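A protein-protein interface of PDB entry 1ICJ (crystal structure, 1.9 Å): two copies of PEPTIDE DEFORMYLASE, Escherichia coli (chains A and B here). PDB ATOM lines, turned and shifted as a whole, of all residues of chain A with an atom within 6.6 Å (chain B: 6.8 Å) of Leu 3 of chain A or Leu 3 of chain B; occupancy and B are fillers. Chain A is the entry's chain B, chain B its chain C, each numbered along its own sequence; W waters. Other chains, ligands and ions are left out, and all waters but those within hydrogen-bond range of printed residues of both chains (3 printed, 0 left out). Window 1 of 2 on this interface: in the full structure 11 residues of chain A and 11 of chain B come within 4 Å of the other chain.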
ATOM      1  N   SER A   1     -20.357  21.606 -25.644  1.00  0.00           N
ATOM      2  CA  SER A   1     -18.938  21.217 -25.485  1.00  0.00           C
ATOM      3  C   SER A   1     -18.170  21.446 -26.782  1.00  0.00           C
ATOM      4  O   SER A   1     -18.727  21.309 -27.869  1.00  0.00           O
ATOM      5  CB  SER A   1     -18.836  19.746 -25.096  1.00  0.00           C
ATOM      6  OG  SER A   1     -19.762  19.440 -24.090  1.00  0.00           O
ATOM      7  N   VAL A   2     -16.889  21.781 -26.649  1.00  0.00           N
ATOM      8  CA  VAL A   2     -15.974  21.876 -27.782  1.00  0.00           C
ATOM      9  C   VAL A   2     -15.265  20.525 -27.968  1.00  0.00           C
ATOM     10  O   VAL A   2     -14.728  19.952 -27.016  1.00  0.00           O
ATOM     11  CB  VAL A   2     -14.932  23.007 -27.559  1.00  0.00           C
ATOM     12  CG1 VAL A   2     -13.892  22.980 -28.644  1.00  0.00           C
ATOM     13  CG2 VAL A   2     -15.627  24.354 -27.516  1.00  0.00           C
ATOM     14  N   LEU A   3     -15.434  19.942 -29.148  1.00  0.00           N
ATOM     15  CA  LEU A   3     -14.873  18.640 -29.466  1.00  0.00           C
ATOM     16  C   LEU A   3     -13.521  18.808 -30.123  1.00  0.00           C
ATOM     17  O   LEU A   3     -13.246  19.838 -30.739  1.00  0.00           O
ATOM     18  CB  LEU A   3     -15.804  17.880 -30.408  1.00  0.00           C
ATOM     19  CG  LEU A   3     -17.286  17.853 -30.037  1.00  0.00           C
ATOM     20  CD1 LEU A   3     -18.072  17.146 -31.099  1.00  0.00           C
ATOM     21  CD2 LEU A   3     -17.471  17.147 -28.726  1.00  0.00           C
ATOM     22  N   GLN A   4     -12.695  17.776 -30.041  1.00  0.00           N
ATOM     23  CA  GLN A   4     -11.401  17.791 -30.704  1.00  0.00           C
ATOM     24  C   GLN A   4     -11.571  17.477 -32.178  1.00  0.00           C
ATOM     25  O   GLN A   4     -12.326  16.569 -32.540  1.00  0.00           O
ATOM     26  CB  GLN A   4     -10.464  16.769 -30.081  1.00  0.00           C
ATOM     27  CG  GLN A   4      -9.047  16.862 -30.600  1.00  0.00           C
ATOM     28  CD  GLN A   4      -8.236  15.607 -30.323  1.00  0.00           C
ATOM     29  OE1 GLN A   4      -8.670  14.480 -30.638  1.00  0.00           O
ATOM     30  NE2 GLN A   4      -7.036  15.790 -29.762  1.00  0.00           N
ATOM     31  N   VAL A   5     -10.938  18.287 -33.027  1.00  0.00           N
ATOM     32  CA  VAL A   5     -11.009  18.100 -34.472  1.00  0.00           C
ATOM     33  C   VAL A   5      -9.812  17.280 -34.923  1.00  0.00           C
ATOM     34  O   VAL A   5      -8.694  17.598 -34.566  1.00  0.00           O
ATOM     35  CB  VAL A   5     -11.032  19.469 -35.223  1.00  0.00           C
ATOM     36  CG1 VAL A   5     -11.090  19.247 -36.734  1.00  0.00           C
ATOM     37  CG2 VAL A   5     -12.232  20.292 -34.774  1.00  0.00           C
ATOM     38  N   ILE A  30     -25.138  16.597 -30.475  1.00  0.00           N
ATOM     39  CA  ILE A  30     -24.028  16.506 -31.412  1.00  0.00           C
ATOM     40  C   ILE A  30     -24.005  17.731 -32.319  1.00  0.00           C
ATOM     41  O   ILE A  30     -22.967  18.367 -32.470  1.00  0.00           O
ATOM     42  CB  ILE A  30     -24.116  15.210 -32.276  1.00  0.00           C
ATOM     43  CG1 ILE A  30     -23.834  13.965 -31.414  1.00  0.00           C
ATOM     44  CG2 ILE A  30     -23.136  15.284 -33.433  1.00  0.00           C
ATOM     45  CD1 ILE A  30     -24.158  12.652 -32.078  1.00  0.00           C
ATOM     46  N   ASP A  33     -22.876  20.765 -30.262  1.00  0.00           N
ATOM     47  CA  ASP A  33     -21.444  20.690 -29.980  1.00  0.00           C
ATOM     48  C   ASP A  33     -20.618  20.987 -31.230  1.00  0.00           C
ATOM     49  O   ASP A  33     -19.539  21.571 -31.130  1.00  0.00           O
ATOM     50  CB  ASP A  33     -21.059  19.304 -29.470  1.00  0.00           C
ATOM     51  CG  ASP A  33     -21.563  19.018 -28.055  1.00  0.00           C
ATOM     52  OD1 ASP A  33     -21.969  19.943 -27.326  1.00  0.00           O
ATOM     53  OD2 ASP A  33     -21.535  17.841 -27.666  1.00  0.00           O
ATOM     54  N   MET A  34     -21.081  20.488 -32.385  1.00  0.00           N
ATOM     55  CA  MET A  34     -20.412  20.741 -33.666  1.00  0.00           C
ATOM     56  C   MET A  34     -20.390  22.223 -34.047  1.00  0.00           C
ATOM     57  O   MET A  34     -19.368  22.715 -34.488  1.00  0.00           O
ATOM     58  CB  MET A  34     -21.051  19.919 -34.795  1.00  0.00           C
ATOM     59  CG  MET A  34     -20.596  18.458 -34.815  1.00  0.00           C
ATOM     60  SD  MET A  34     -21.453  17.491 -36.046  1.00  0.00           S
ATOM     61  CE  MET A  34     -20.820  18.177 -37.543  1.00  0.00           C
ATOM     62  N   GLU A  36     -20.572  24.679 -31.794  1.00  0.00           N
ATOM     63  CA  GLU A  36     -19.685  25.242 -30.777  1.00  0.00           C
ATOM     64  C   GLU A  36     -18.208  25.042 -31.150  1.00  0.00           C
ATOM     65  O   GLU A  36     -17.405  25.981 -31.069  1.00  0.00           O
ATOM     66  CB  GLU A  36     -19.998  24.610 -29.419  1.00  0.00           C
ATOM     67  CG  GLU A  36     -19.152  25.137 -28.303  1.00  0.00           C
ATOM     68  CD  GLU A  36     -19.827  25.082 -26.939  1.00  0.00           C
ATOM     69  OE1 GLU A  36     -20.754  24.277 -26.736  1.00  0.00           O
ATOM     70  OE2 GLU A  36     -19.416  25.862 -26.063  1.00  0.00           O
ATOM     71  N   THR A  37     -17.895  23.866 -31.691  1.00  0.00           N
ATOM     72  CA  THR A  37     -16.532  23.533 -32.117  1.00  0.00           C
ATOM     73  C   THR A  37     -16.118  24.359 -33.341  1.00  0.00           C
ATOM     74  O   THR A  37     -15.015  24.896 -33.396  1.00  0.00           O
ATOM     75  CB  THR A  37     -16.422  22.029 -32.457  1.00  0.00           C
ATOM     76  OG1 THR A  37     -16.843  21.260 -31.325  1.00  0.00           O
ATOM     77  CG2 THR A  37     -14.997  21.644 -32.819  1.00  0.00           C
ATOM     78  N   GLU A  41     -13.015  27.107 -33.401  1.00  0.00           N
ATOM     79  CA  GLU A  41     -11.902  26.976 -34.337  1.00  0.00           C
ATOM     80  C   GLU A  41     -11.969  27.956 -35.514  1.00  0.00           C
ATOM     81  O   GLU A  41     -11.086  27.935 -36.365  1.00  0.00           O
ATOM     82  CB  GLU A  41     -11.853  25.540 -34.879  1.00  0.00           C
ATOM     83  CG  GLU A  41     -11.861  24.449 -33.808  1.00  0.00           C
ATOM     84  CD  GLU A  41     -10.473  23.929 -33.475  1.00  0.00           C
ATOM     85  OE1 GLU A  41      -9.771  23.446 -34.391  1.00  0.00           O
ATOM     86  OE2 GLU A  41     -10.085  23.984 -32.288  1.00  0.00           O
ATOM     87  N   LEU A  46     -18.263  22.170 -40.826  1.00  0.00           N
ATOM     88  CA  LEU A  46     -17.697  21.036 -40.091  1.00  0.00           C
ATOM     89  C   LEU A  46     -18.572  19.802 -40.314  1.00  0.00           C
ATOM     90  O   LEU A  46     -19.805  19.893 -40.298  1.00  0.00           O
ATOM     91  CB  LEU A  46     -17.614  21.377 -38.592  1.00  0.00           C
ATOM     92  CG  LEU A  46     -16.946  20.352 -37.666  1.00  0.00           C
ATOM     93  CD1 LEU A  46     -15.469  20.361 -37.918  1.00  0.00           C
ATOM     94  CD2 LEU A  46     -17.220  20.686 -36.223  1.00  0.00           C
ATOM     95  N   VAL A  51     -14.907  15.113 -36.203  1.00  0.00           N
ATOM     96  CA  VAL A  51     -14.861  15.031 -34.740  1.00  0.00           C
ATOM     97  C   VAL A  51     -15.093  13.597 -34.248  1.00  0.00           C
ATOM     98  O   VAL A  51     -15.399  13.378 -33.073  1.00  0.00           O
ATOM     99  CB  VAL A  51     -15.878  16.030 -34.075  1.00  0.00           C
ATOM    100  CG1 VAL A  51     -15.455  17.471 -34.371  1.00  0.00           C
ATOM    101  CG2 VAL A  51     -17.322  15.768 -34.538  1.00  0.00           C
ATOM    102  N   ILE A  53     -17.268  11.305 -35.174  1.00  0.00           N
ATOM    103  CA  ILE A  53     -18.634  10.838 -35.107  1.00  0.00           C
ATOM    104  C   ILE A  53     -19.073  10.475 -36.524  1.00  0.00           C
ATOM    105  O   ILE A  53     -19.223  11.340 -37.378  1.00  0.00           O
ATOM    106  CB  ILE A  53     -19.562  11.927 -34.560  1.00  0.00           C
ATOM    107  CG1 ILE A  53     -19.182  12.267 -33.106  1.00  0.00           C
ATOM    108  CG2 ILE A  53     -21.019  11.457 -34.652  1.00  0.00           C
ATOM    109  CD1 ILE A  53     -19.809  13.553 -32.572  1.00  0.00           C
ATOM    110  N   SER B   1     -15.565  10.879 -28.885  1.00  0.00           N
ATOM    111  CA  SER B   1     -14.944  12.199 -29.118  1.00  0.00           C
ATOM    112  C   SER B   1     -14.216  12.652 -27.869  1.00  0.00           C
ATOM    113  O   SER B   1     -14.608  12.314 -26.750  1.00  0.00           O
ATOM    114  CB  SER B   1     -16.014  13.225 -29.492  1.00  0.00           C
ATOM    115  OG  SER B   1     -16.885  12.698 -30.476  1.00  0.00           O
ATOM    116  N   VAL B   2     -13.152  13.417 -28.069  1.00  0.00           N
ATOM    117  CA  VAL B   2     -12.430  14.038 -26.972  1.00  0.00           C
ATOM    118  C   VAL B   2     -12.991  15.446 -26.774  1.00  0.00           C
ATOM    119  O   VAL B   2     -13.127  16.201 -27.733  1.00  0.00           O
ATOM    120  CB  VAL B   2     -10.900  14.084 -27.270  1.00  0.00           C
ATOM    121  CG1 VAL B   2     -10.158  14.919 -26.225  1.00  0.00           C
ATOM    122  CG2 VAL B   2     -10.340  12.668 -27.315  1.00  0.00           C
ATOM    123  N   LEU B   3     -13.454  15.724 -25.556  1.00  0.00           N
ATOM    124  CA  LEU B   3     -14.076  16.994 -25.221  1.00  0.00           C
ATOM    125  C   LEU B   3     -13.044  17.914 -24.607  1.00  0.00           C
ATOM    126  O   LEU B   3     -12.066  17.442 -24.028  1.00  0.00           O
ATOM    127  CB  LEU B   3     -15.210  16.777 -24.224  1.00  0.00           C
ATOM    128  CG  LEU B   3     -16.226  15.674 -24.555  1.00  0.00           C
ATOM    129  CD1 LEU B   3     -17.221  15.527 -23.424  1.00  0.00           C
ATOM    130  CD2 LEU B   3     -16.944  16.007 -25.812  1.00  0.00           C
ATOM    131  N   GLN B   4     -13.282  19.221 -24.703  1.00  0.00           N
ATOM    132  CA  GLN B   4     -12.392  20.197 -24.101  1.00  0.00           C
ATOM    133  C   GLN B   4     -12.669  20.271 -22.612  1.00  0.00           C
ATOM    134  O   GLN B   4     -13.821  20.301 -22.195  1.00  0.00           O
ATOM    135  CB  GLN B   4     -12.594  21.572 -24.744  1.00  0.00           C
ATOM    136  CG  GLN B   4     -11.585  22.606 -24.297  1.00  0.00           C
ATOM    137  CD  GLN B   4     -12.043  24.036 -24.563  1.00  0.00           C
ATOM    138  OE1 GLN B   4     -13.165  24.429 -24.217  1.00  0.00           O
ATOM    139  NE2 GLN B   4     -11.159  24.826 -25.149  1.00  0.00           N
ATOM    140  N   VAL B   5     -11.605  20.226 -21.816  1.00  0.00           N
ATOM    141  CA  VAL B   5     -11.718  20.349 -20.366  1.00  0.00           C
ATOM    142  C   VAL B   5     -11.538  21.799 -19.945  1.00  0.00           C
ATOM    143  O   VAL B   5     -10.581  22.447 -20.348  1.00  0.00           O
ATOM    144  CB  VAL B   5     -10.662  19.457 -19.664  1.00  0.00           C
ATOM    145  CG1 VAL B   5     -10.756  19.586 -18.142  1.00  0.00           C
ATOM    146  CG2 VAL B   5     -10.869  18.001 -20.081  1.00  0.00           C
ATOM    147  N   ARG B  29     -23.523   8.186 -24.462  1.00  0.00           N
ATOM    148  CA  ARG B  29     -22.576   8.810 -25.362  1.00  0.00           C
ATOM    149  C   ARG B  29     -21.675   9.788 -24.601  1.00  0.00           C
ATOM    150  O   ARG B  29     -20.448   9.745 -24.727  1.00  0.00           O
ATOM    151  CB  ARG B  29     -23.352   9.522 -26.461  1.00  0.00           C
ATOM    152  CG  ARG B  29     -22.516  10.296 -27.408  1.00  0.00           C
ATOM    153  CD  ARG B  29     -23.295  10.549 -28.671  1.00  0.00           C
ATOM    154  NE  ARG B  29     -22.400  10.462 -29.801  1.00  0.00           N
ATOM    155  CZ  ARG B  29     -22.295   9.423 -30.611  1.00  0.00           C
ATOM    156  NH1 ARG B  29     -23.353   8.678 -30.902  1.00  0.00           N
ATOM    157  NH2 ARG B  29     -21.191   9.304 -31.317  1.00  0.00           N
ATOM    158  N   ILE B  30     -22.285  10.586 -23.732  1.00  0.00           N
ATOM    159  CA  ILE B  30     -21.563  11.480 -22.845  1.00  0.00           C
ATOM    160  C   ILE B  30     -20.561  10.703 -21.979  1.00  0.00           C
ATOM    161  O   ILE B  30     -19.400  11.080 -21.885  1.00  0.00           O
ATOM    162  CB  ILE B  30     -22.550  12.259 -21.930  1.00  0.00           C
ATOM    163  CG1 ILE B  30     -23.357  13.269 -22.766  1.00  0.00           C
ATOM    164  CG2 ILE B  30     -21.785  12.988 -20.821  1.00  0.00           C
ATOM    165  CD1 ILE B  30     -24.536  13.891 -22.044  1.00  0.00           C
ATOM    166  N   ASP B  33     -17.628   9.573 -24.125  1.00  0.00           N
ATOM    167  CA  ASP B  33     -16.776  10.698 -24.484  1.00  0.00           C
ATOM    168  C   ASP B  33     -15.963  11.145 -23.287  1.00  0.00           C
ATOM    169  O   ASP B  33     -14.843  11.611 -23.444  1.00  0.00           O
ATOM    170  CB  ASP B  33     -17.607  11.884 -24.965  1.00  0.00           C
ATOM    171  CG  ASP B  33     -18.218  11.670 -26.360  1.00  0.00           C
ATOM    172  OD1 ASP B  33     -17.812  10.740 -27.096  1.00  0.00           O
ATOM    173  OD2 ASP B  33     -19.084  12.486 -26.726  1.00  0.00           O
ATOM    174  N   MET B  34     -16.574  11.105 -22.103  1.00  0.00           N
ATOM    175  CA  MET B  34     -15.878  11.464 -20.870  1.00  0.00           C
ATOM    176  C   MET B  34     -14.720  10.519 -20.540  1.00  0.00           C
ATOM    177  O   MET B  34     -13.644  10.964 -20.155  1.00  0.00           O
ATOM    178  CB  MET B  34     -16.867  11.507 -19.709  1.00  0.00           C
ATOM    179  CG  MET B  34     -17.616  12.823 -19.608  1.00  0.00           C
ATOM    180  SD  MET B  34     -18.862  12.784 -18.310  1.00  0.00           S
ATOM    181  CE  MET B  34     -17.789  12.713 -16.859  1.00  0.00           C
ATOM    182  N   GLU B  36     -13.071   8.753 -22.842  1.00  0.00           N
ATOM    183  CA  GLU B  36     -12.118   9.068 -23.901  1.00  0.00           C
ATOM    184  C   GLU B  36     -11.304  10.324 -23.585  1.00  0.00           C
ATOM    185  O   GLU B  36     -10.092  10.329 -23.743  1.00  0.00           O
ATOM    186  CB  GLU B  36     -12.865   9.226 -25.228  1.00  0.00           C
ATOM    187  CG  GLU B  36     -11.980   9.528 -26.400  1.00  0.00           C
ATOM    188  CD  GLU B  36     -12.552   9.031 -27.718  1.00  0.00           C
ATOM    189  OE1 GLU B  36     -13.778   8.837 -27.834  1.00  0.00           O
ATOM    190  OE2 GLU B  36     -11.740   8.791 -28.629  1.00  0.00           O
ATOM    191  N   THR B  37     -11.964  11.335 -23.037  1.00  0.00           N
ATOM    192  CA  THR B  37     -11.318  12.574 -22.662  1.00  0.00           C
ATOM    193  C   THR B  37     -10.353  12.346 -21.479  1.00  0.00           C
ATOM    194  O   THR B  37      -9.209  12.836 -21.495  1.00  0.00           O
ATOM    195  CB  THR B  37     -12.366  13.638 -22.278  1.00  0.00           C
ATOM    196  OG1 THR B  37     -13.260  13.819 -23.373  1.00  0.00           O
ATOM    197  CG2 THR B  37     -11.716  14.968 -21.950  1.00  0.00           C
ATOM    198  N   GLU B  41      -6.277  12.819 -21.526  1.00  0.00           N
ATOM    199  CA  GLU B  41      -5.635  13.800 -20.656  1.00  0.00           C
ATOM    200  C   GLU B  41      -4.814  13.141 -19.559  1.00  0.00           C
ATOM    201  O   GLU B  41      -4.231  13.818 -18.713  1.00  0.00           O
ATOM    202  CB  GLU B  41      -6.692  14.683 -20.007  1.00  0.00           C
ATOM    203  CG  GLU B  41      -7.536  15.463 -20.990  1.00  0.00           C
ATOM    204  CD  GLU B  41      -6.870  16.746 -21.395  1.00  0.00           C
ATOM    205  OE1 GLU B  41      -7.007  17.748 -20.651  1.00  0.00           O
ATOM    206  OE2 GLU B  41      -6.151  16.726 -22.415  1.00  0.00           O
ATOM    207  N   LEU B  46     -13.031  12.293 -13.827  1.00  0.00           N
ATOM    208  CA  LEU B  46     -13.544  13.438 -14.558  1.00  0.00           C
ATOM    209  C   LEU B  46     -15.030  13.575 -14.265  1.00  0.00           C
ATOM    210  O   LEU B  46     -15.745  12.575 -14.243  1.00  0.00           O
ATOM    211  CB  LEU B  46     -13.327  13.235 -16.064  1.00  0.00           C
ATOM    212  CG  LEU B  46     -13.692  14.405 -16.989  1.00  0.00           C
ATOM    213  CD1 LEU B  46     -12.692  15.520 -16.820  1.00  0.00           C
ATOM    214  CD2 LEU B  46     -13.698  13.933 -18.443  1.00  0.00           C
ATOM    215  N   ALA B  48     -18.754  15.610 -15.204  1.00  0.00           N
ATOM    216  CA  ALA B  48     -19.386  16.196 -16.384  1.00  0.00           C
ATOM    217  C   ALA B  48     -19.238  17.715 -16.435  1.00  0.00           C
ATOM    218  O   ALA B  48     -19.017  18.279 -17.507  1.00  0.00           O
ATOM    219  CB  ALA B  48     -20.845  15.809 -16.450  1.00  0.00           C
ATOM    220  N   VAL B  51     -16.399  19.341 -18.441  1.00  0.00           N
ATOM    221  CA  VAL B  51     -16.509  19.415 -19.897  1.00  0.00           C
ATOM    222  C   VAL B  51     -17.758  20.181 -20.337  1.00  0.00           C
ATOM    223  O   VAL B  51     -18.210  20.035 -21.464  1.00  0.00           O
ATOM    224  CB  VAL B  51     -16.504  17.997 -20.531  1.00  0.00           C
ATOM    225  CG1 VAL B  51     -15.160  17.352 -20.306  1.00  0.00           C
ATOM    226  CG2 VAL B  51     -17.618  17.115 -19.954  1.00  0.00           C
ATOM    227  N   ILE B  53     -20.914  19.996 -19.212  1.00  0.00           N
ATOM    228  CA  ILE B  53     -22.168  19.242 -19.207  1.00  0.00           C
ATOM    229  C   ILE B  53     -22.674  19.178 -17.759  1.00  0.00           C
ATOM    230  O   ILE B  53     -22.012  18.626 -16.885  1.00  0.00           O
ATOM    231  CB  ILE B  53     -21.950  17.819 -19.747  1.00  0.00           C
ATOM    232  CG1 ILE B  53     -21.472  17.883 -21.204  1.00  0.00           C
ATOM    233  CG2 ILE B  53     -23.243  17.018 -19.694  1.00  0.00           C
ATOM    234  CD1 ILE B  53     -20.987  16.545 -21.740  1.00  0.00           C
HETATM  235  O   HOH W   1     -15.872  23.460 -23.781  1.00  0.00           O
HETATM  236  O   HOH W   2     -13.386  14.389 -31.105  1.00  0.00           O
HETATM  237  O   HOH W   3     -16.156  20.787 -23.473  1.00  0.00           O
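Water W3 lies within hydrogen-bond range of the backbone carbonyl oxygen (O) of Gln 4 of chain B (2.7 Å), the backbone carbonyl oxygen (O) of Val 51 of chain B (3.0 Å) and the backbone NH (N) of Val 2 of chain A (3.4 Å). Water W2 lies within hydrogen-bond range of the backbone carbonyl oxygen of Gln 4 of chain A, the backbone carbonyl oxygen of Val 51 of chain A and the backbone NH of Val 2 of chain B. Water W1 bridges the side-chain amide oxygen of Gln 4 of chain B (2.9 Å) and the backbone NH of Val 2 of chain A (3.5 Å).
N of Gln 4 of chain A sits at hydrogen-bond distance from O of Val 2 of chain B. The backbone NH of Gln 4 of chain B is in hydrogen-bond range of the backbone carbonyl oxygen of Val 2 of chain A, 2.8 Å away. The side-chain hydroxyl of Ser 1 of chain A sits at hydrogen-bond distance from the backbone carbonyl oxygen of Val 51 of chain B, 3.1 Å away. The side-chain hydroxyl of Ser 1 of chain B lies within hydrogen-bond range of the backbone carbonyl oxygen of Val 51 of chain A, at 3.1 Å.
Ser 1 of chain A touches Val 51 of chain B, and with the chains exchanged Val 51 of chain A touches Ser 1 of chain B. Ser 1 of chain A touches Ile 53 of chain B, and with the chains exchanged Ile 53 of chain A touches Ser 1 of chain B. Val 2 of chain A touches Leu 3 of chain B, and with the chains exchanged Leu 3 of chain A touches Val 2 of chain B. Val 2 of chain A touches Gln 4 of chain B, and with the chains exchanged Gln 4 of chain A touches Val 2 of chain B. Positions printed for both chains: 1, 2, 3, 4, 5, 30, 33, 34, 36, 37, 41, 46, 51 and 53.
Ile 53 of chain B touches Ser 1 of chain A (CG1 to OG, 3.7 Å). CA of Leu 3 of chain B touches O of Val 2 of chain A, at 3.5 Å. Leu 3 of chain A touches Val 2 of chain B (CA to O, 3.5 Å). Leu 3 of chain A touches Leu 3 of chain B. Ile 30 of chain A touches Arg 29 of chain B (CD1 to NE, 3.6 Å). CG1 of Ile 53 of chain A touches OG of Ser 1 of chain B (3.5 Å). Arg 29 of chain B touches Ile 53 of chain A.
Of the printed residues of chain B, Ser 1 of chain A touches Val 51 (3.1 Å) and Ile 53 (3.7 Å). Of the printed residues of chain B, Val 2 of chain A touches Leu 3 (3.5 Å) and Gln 4 (2.8 Å). Printed residues of chain B within 4 Å of Leu 3 of chain A: Val 2 and Leu 3. Val 5 of chain A touches none of the printed residues of chain B. Glu 41 of chain A touches none of the printed residues of chain B. Printed residues of chain B within 4 Å of Val 51 of chain A: Ser 1. Leu 3 of chain B touches just these residues of chain A: Val 2 (3.5 Å) and Leu 3 (3.2 Å). The nearest residue of chain A that does not touch Leu 3 of chain B is Ser 1 of chain A (4.3 Å). The nearest printed residue of chain B that does not touch Val 2 of chain A is Val 2 of chain B (4.1 Å).
Of the 16 printed residues of chain B, 7 touch a printed residue of chain A. Along chain A the printed residues that touch a printed residue of chain B span positions 1 to 53. Among the printed residues, 11 pairs touch across the chains. Among the printed residues, no Asp or Glu carboxylate lies within 4 Å of a Lys or Arg side-chain nitrogen of the other chain.
N of Ile 53 of chain B lies within hydrogen-bond range of O of Ala 48 of chain B, 3.1 Å away. The side-chain hydroxyl (OG1) of Thr 37 of chain A sits at hydrogen-bond distance from the backbone NH (N) of Leu 3 of chain A, 2.9 Å away. N of Ser 1 of chain B is in hydrogen-bond range of OD1 of Asp 33 of chain B (2.9 Å). The backbone NH (N) of Ser 1 of chain A is in hydrogen-bond range of the side-chain carboxylate (OD1) of Asp 33 of chain A, at 2.9 Å. The backbone NH of Ser 1 of chain B lies within hydrogen-bond range of the side-chain carboxylate of Glu 36 of chain B (2.9 Å). The backbone NH (N) of Leu 3 of chain B lies within hydrogen-bond range of the side-chain hydroxyl (OG1) of Thr 37 of chain B (2.9 Å).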
